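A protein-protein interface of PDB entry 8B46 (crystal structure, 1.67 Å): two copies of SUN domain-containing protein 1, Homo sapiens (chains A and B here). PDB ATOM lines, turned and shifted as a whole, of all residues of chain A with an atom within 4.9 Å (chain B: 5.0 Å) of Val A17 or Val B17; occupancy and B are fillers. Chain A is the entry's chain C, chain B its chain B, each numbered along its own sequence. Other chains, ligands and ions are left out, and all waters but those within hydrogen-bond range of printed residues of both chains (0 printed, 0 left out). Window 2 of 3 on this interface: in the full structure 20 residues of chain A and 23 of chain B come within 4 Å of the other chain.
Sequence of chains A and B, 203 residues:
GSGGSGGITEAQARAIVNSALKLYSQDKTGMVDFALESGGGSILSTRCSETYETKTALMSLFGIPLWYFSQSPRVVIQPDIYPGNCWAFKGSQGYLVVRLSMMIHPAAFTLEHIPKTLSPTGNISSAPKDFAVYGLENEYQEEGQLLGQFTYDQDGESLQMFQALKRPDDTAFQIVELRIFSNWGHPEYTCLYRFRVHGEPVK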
ATOM      1  N   ALA A  13     -19.992  21.196   1.062  1.00  0.00           N
ATOM      2  CA  ALA A  13     -20.587  20.200   1.945  1.00  0.00           C
ATOM      3  C   ALA A  13     -20.391  20.582   3.400  1.00  0.00           C
ATOM      4  O   ALA A  13     -21.346  20.584   4.188  1.00  0.00           O
ATOM      5  CB  ALA A  13     -19.958  18.836   1.683  1.00  0.00           C
ATOM      6  N   ARG A  14     -19.158  20.939   3.761  1.00  0.00           N
ATOM      7  CA  ARG A  14     -18.900  21.351   5.132  1.00  0.00           C
ATOM      8  C   ARG A  14     -19.726  22.576   5.485  1.00  0.00           C
ATOM      9  O   ARG A  14     -20.210  22.691   6.607  1.00  0.00           O
ATOM     10  CB  ARG A  14     -17.410  21.609   5.343  1.00  0.00           C
ATOM     11  CG  ARG A  14     -16.526  20.467   4.824  1.00  0.00           C
ATOM     12  CD  ARG A  14     -15.080  20.568   5.327  1.00  0.00           C
ATOM     13  NE  ARG A  14     -14.859  19.582   6.373  1.00  0.00           N
ATOM     14  CZ  ARG A  14     -14.421  18.354   6.153  1.00  0.00           C
ATOM     15  NH1 ARG A  14     -14.079  17.957   4.938  1.00  0.00           N
ATOM     16  NH2 ARG A  14     -14.354  17.495   7.171  1.00  0.00           N
ATOM     17  N   ALA A  15     -19.913  23.494   4.528  1.00  0.00           N
ATOM     18  CA  ALA A  15     -20.742  24.670   4.785  1.00  0.00           C
ATOM     19  C   ALA A  15     -22.187  24.290   5.075  1.00  0.00           C
ATOM     20  O   ALA A  15     -22.816  24.843   5.986  1.00  0.00           O
ATOM     21  CB  ALA A  15     -20.695  25.612   3.588  1.00  0.00           C
ATOM     22  N   ILE A  16     -22.741  23.373   4.286  1.00  0.00           N
ATOM     23  CA  ILE A  16     -24.108  22.930   4.518  1.00  0.00           C
ATOM     24  C   ILE A  16     -24.218  22.282   5.882  1.00  0.00           C
ATOM     25  O   ILE A  16     -25.155  22.552   6.651  1.00  0.00           O
ATOM     26  CB  ILE A  16     -24.556  21.974   3.401  1.00  0.00           C
ATOM     27  CG1 ILE A  16     -24.698  22.744   2.092  1.00  0.00           C
ATOM     28  CG2 ILE A  16     -25.825  21.215   3.791  1.00  0.00           C
ATOM     29  CD1 ILE A  16     -25.039  21.851   0.940  1.00  0.00           C
ATOM     30  N   VAL A  17     -23.251  21.421   6.201  1.00  0.00           N
ATOM     31  CA  VAL A  17     -23.282  20.703   7.466  1.00  0.00           C
ATOM     32  C   VAL A  17     -23.220  21.687   8.626  1.00  0.00           C
ATOM     33  O   VAL A  17     -24.040  21.633   9.561  1.00  0.00           O
ATOM     34  CB  VAL A  17     -22.129  19.680   7.521  1.00  0.00           C
ATOM     35  CG1 VAL A  17     -22.116  18.980   8.832  1.00  0.00           C
ATOM     36  CG2 VAL A  17     -22.307  18.654   6.450  1.00  0.00           C
ATOM     37  N   ASN A  18     -22.284  22.644   8.550  1.00  0.00           N
ATOM     38  CA  ASN A  18     -22.092  23.587   9.650  1.00  0.00           C
ATOM     39  C   ASN A  18     -23.292  24.496   9.797  1.00  0.00           C
ATOM     40  O   ASN A  18     -23.681  24.826  10.913  1.00  0.00           O
ATOM     41  CB  ASN A  18     -20.821  24.419   9.453  1.00  0.00           C
ATOM     42  CG  ASN A  18     -19.557  23.559   9.480  1.00  0.00           C
ATOM     43  OD1 ASN A  18     -19.512  22.507  10.129  1.00  0.00           O
ATOM     44  ND2 ASN A  18     -18.526  24.009   8.786  1.00  0.00           N
ATOM     45  N   SER A  19     -23.877  24.927   8.682  1.00  0.00           N
ATOM     46  CA  SER A  19     -25.069  25.762   8.751  1.00  0.00           C
ATOM     47  C   SER A  19     -26.231  25.015   9.416  1.00  0.00           C
ATOM     48  O   SER A  19     -26.954  25.584  10.251  1.00  0.00           O
ATOM     49  CB  SER A  19     -25.401  26.252   7.332  1.00  0.00           C
ATOM     50  OG  SER A  19     -26.557  27.070   7.315  1.00  0.00           O
ATOM     51  N   ALA A  20     -26.428  23.734   9.071  1.00  0.00           N
ATOM     52  CA  ALA A  20     -27.497  22.966   9.724  1.00  0.00           C
ATOM     53  C   ALA A  20     -27.231  22.769  11.218  1.00  0.00           C
ATOM     54  O   ALA A  20     -28.154  22.865  12.039  1.00  0.00           O
ATOM     55  CB  ALA A  20     -27.700  21.616   9.039  1.00  0.00           C
ATOM     56  N   LEU A  21     -25.983  22.475  11.596  1.00  0.00           N
ATOM     57  CA  LEU A  21     -25.696  22.314  13.022  1.00  0.00           C
ATOM     58  C   LEU A  21     -25.865  23.622  13.769  1.00  0.00           C
ATOM     59  O   LEU A  21     -26.336  23.629  14.910  1.00  0.00           O
ATOM     60  CB  LEU A  21     -24.283  21.782  13.250  1.00  0.00           C
ATOM     61  CG  LEU A  21     -24.215  20.262  13.213  1.00  0.00           C
ATOM     62  CD1 LEU A  21     -22.779  19.788  13.343  1.00  0.00           C
ATOM     63  CD2 LEU A  21     -25.032  19.763  14.357  1.00  0.00           C
ATOM     64  N   ALA B  13     -27.182  16.211  -0.464  1.00  0.00           N
ATOM     65  CA  ALA B  13     -26.395  16.537   0.721  1.00  0.00           C
ATOM     66  C   ALA B  13     -27.281  17.069   1.835  1.00  0.00           C
ATOM     67  O   ALA B  13     -27.170  16.643   2.995  1.00  0.00           O
ATOM     68  CB  ALA B  13     -25.323  17.560   0.383  1.00  0.00           C
ATOM     69  N   ARG B  14     -28.175  18.002   1.501  1.00  0.00           N
ATOM     70  CA  ARG B  14     -29.079  18.518   2.518  1.00  0.00           C
ATOM     71  C   ARG B  14     -29.929  17.394   3.095  1.00  0.00           C
ATOM     72  O   ARG B  14     -30.183  17.369   4.301  1.00  0.00           O
ATOM     73  CB  ARG B  14     -29.947  19.636   1.949  1.00  0.00           C
ATOM     74  CG  ARG B  14     -29.148  20.698   1.218  1.00  0.00           C
ATOM     75  CD  ARG B  14     -29.975  21.943   0.935  1.00  0.00           C
ATOM     76  NE  ARG B  14     -29.590  23.052   1.797  1.00  0.00           N
ATOM     77  CZ  ARG B  14     -28.691  23.972   1.477  1.00  0.00           C
ATOM     78  NH1 ARG B  14     -28.103  23.979   0.291  1.00  0.00           N
ATOM     79  NH2 ARG B  14     -28.383  24.917   2.364  1.00  0.00           N
ATOM     80  N   ALA B  15     -30.350  16.437   2.261  1.00  0.00           N
ATOM     81  CA  ALA B  15     -31.124  15.303   2.766  1.00  0.00           C
ATOM     82  C   ALA B  15     -30.311  14.430   3.714  1.00  0.00           C
ATOM     83  O   ALA B  15     -30.837  13.955   4.729  1.00  0.00           O
ATOM     84  CB  ALA B  15     -31.656  14.466   1.612  1.00  0.00           C
ATOM     85  N   ILE B  16     -29.047  14.166   3.380  1.00  0.00           N
ATOM     86  CA  ILE B  16     -28.200  13.366   4.267  1.00  0.00           C
ATOM     87  C   ILE B  16     -28.068  14.051   5.619  1.00  0.00           C
ATOM     88  O   ILE B  16     -28.244  13.433   6.680  1.00  0.00           O
ATOM     89  CB  ILE B  16     -26.817  13.139   3.635  1.00  0.00           C
ATOM     90  CG1 ILE B  16     -26.933  12.277   2.381  1.00  0.00           C
ATOM     91  CG2 ILE B  16     -25.871  12.480   4.620  1.00  0.00           C
ATOM     92  CD1 ILE B  16     -27.644  10.987   2.650  1.00  0.00           C
ATOM     93  N   VAL B  17     -27.792  15.359   5.587  1.00  0.00           N
ATOM     94  CA  VAL B  17     -27.594  16.133   6.806  1.00  0.00           C
ATOM     95  C   VAL B  17     -28.869  16.171   7.646  1.00  0.00           C
ATOM     96  O   VAL B  17     -28.836  16.007   8.877  1.00  0.00           O
ATOM     97  CB  VAL B  17     -27.116  17.545   6.436  1.00  0.00           C
ATOM     98  CG1 VAL B  17     -26.940  18.366   7.673  1.00  0.00           C
ATOM     99  CG2 VAL B  17     -25.823  17.463   5.654  1.00  0.00           C
ATOM    100  N   ASN B  18     -30.009  16.416   7.007  1.00  0.00           N
ATOM    101  CA  ASN B  18     -31.248  16.496   7.770  1.00  0.00           C
ATOM    102  C   ASN B  18     -31.591  15.142   8.363  1.00  0.00           C
ATOM    103  O   ASN B  18     -32.064  15.070   9.492  1.00  0.00           O
ATOM    104  CB  ASN B  18     -32.382  17.030   6.892  1.00  0.00           C
ATOM    105  CG  ASN B  18     -32.133  18.485   6.434  1.00  0.00           C
ATOM    106  OD1 ASN B  18     -31.515  19.302   7.143  1.00  0.00           O
ATOM    107  ND2 ASN B  18     -32.563  18.786   5.220  1.00  0.00           N
ATOM    108  N   SER B  19     -31.356  14.052   7.634  1.00  0.00           N
ATOM    109  CA  SER B  19     -31.634  12.743   8.217  1.00  0.00           C
ATOM    110  C   SER B  19     -30.762  12.486   9.426  1.00  0.00           C
ATOM    111  O   SER B  19     -31.251  12.017  10.467  1.00  0.00           O
ATOM    112  CB  SER B  19     -31.436  11.643   7.173  1.00  0.00           C
ATOM    113  OG  SER B  19     -31.953  12.101   5.942  1.00  0.00           O
ATOM    114  N   ALA B  20     -29.468  12.803   9.320  1.00  0.00           N
ATOM    115  CA  ALA B  20     -28.575  12.584  10.458  1.00  0.00           C
ATOM    116  C   ALA B  20     -28.979  13.433  11.667  1.00  0.00           C
ATOM    117  O   ALA B  20     -28.943  12.963  12.809  1.00  0.00           O
ATOM    118  CB  ALA B  20     -27.146  12.897  10.038  1.00  0.00           C
ATOM    119  N   LEU B  21     -29.344  14.702  11.437  1.00  0.00           N
ATOM    120  CA  LEU B  21     -29.781  15.545  12.537  1.00  0.00           C
ATOM    121  C   LEU B  21     -31.104  15.062  13.116  1.00  0.00           C
ATOM    122  O   LEU B  21     -31.305  15.139  14.330  1.00  0.00           O
ATOM    123  CB  LEU B  21     -29.911  16.999  12.092  1.00  0.00           C
ATOM    124  CG  LEU B  21     -28.654  17.858  12.127  1.00  0.00           C
ATOM    125  CD1 LEU B  21     -28.899  19.319  11.617  1.00  0.00           C
ATOM    126  CD2 LEU B  21     -28.107  17.879  13.502  1.00  0.00           C
ATOM    127  N   LYS B  22     -32.020  14.566  12.275  1.00  0.00           N
ATOM    128  CA  LYS B  22     -33.295  14.063  12.795  1.00  0.00           C
ATOM    129  C   LYS B  22     -33.071  12.892  13.739  1.00  0.00           C
ATOM    130  O   LYS B  22     -33.584  12.867  14.871  1.00  0.00           O
ATOM    131  CB  LYS B  22     -34.195  13.638  11.639  1.00  0.00           C
ATOM    132  CG  LYS B  22     -35.528  13.034  12.090  1.00  0.00           C
ATOM    133  CD  LYS B  22     -36.438  12.829  10.841  1.00  0.00           C
ATOM    134  CE  LYS B  22     -37.822  12.403  11.281  1.00  0.00           C
ATOM    135  NZ  LYS B  22     -38.753  12.344  10.151  1.00  0.00           N
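Ile A16 touches Arg B14, but with the chains exchanged Arg A14 does not touch Ile B16 (10.8 Å). Val A17 touches its own counterpart, Val B17. Ala A20 touches Val B17, but with the chains exchanged Val A17 does not touch Ala B20 (8.0 Å). Ala A20 touches Leu B21, but with the chains exchanged Leu A21 does not touch Ala B20 (7.9 Å). Of the 5 pairs that touch across the chains among the printed residues, 2 have their exchanged pair printed and touching as well.
Printed residues of chain B that touch a printed residue of chain A: Arg B14, Val B17 and Leu B21. Hydrophobic or aromatic side chains of chain B that line the printed part of chain A: Val B17 and Leu B21. Among the printed residues, no Asp or Glu carboxylate lies within 4 Å of a Lys or Arg side-chain nitrogen of the other chain.
The side-chain amide nitrogen of Asn B18 lies within hydrogen-bond range of the backbone carbonyl oxygen of Arg B14, at 2.9 Å.
Arg B14 touches Ile A16. CG2 of Val A17 touches CG2 of Val B17, 3.8 Å away. Val B17 touches Ala A20 (CG1 to CB, 3.6 Å). Leu B21 touches Ala A20 (CD1 to O, 3.6 Å). Leu A21 touches Leu B21 (CD2 to CD2, 3.7 Å).
Printed residues of chain B within 4 Å of Val A17: Val B17. Val B17 touches just these residues of chain A: Val A17 and Ala A20. Of the printed residues of chain A, Arg B14 touches Ile A16 (3.8 Å). Printed residues of chain B within 4 Å of Leu A21: Leu B21 (3.7 Å). Printed residues of chain A within 4 Å of Leu B21: Ala A20 and Leu A21. Printed residues of chain B within 4 Å of Ala A20: Val B17 and Leu B21. Of the printed residues of chain B, Ile A16 touches Arg B14 (3.8 Å). The nearest printed residue of chain B that does not touch Ile A16 is Val B17 (4.2 Å).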
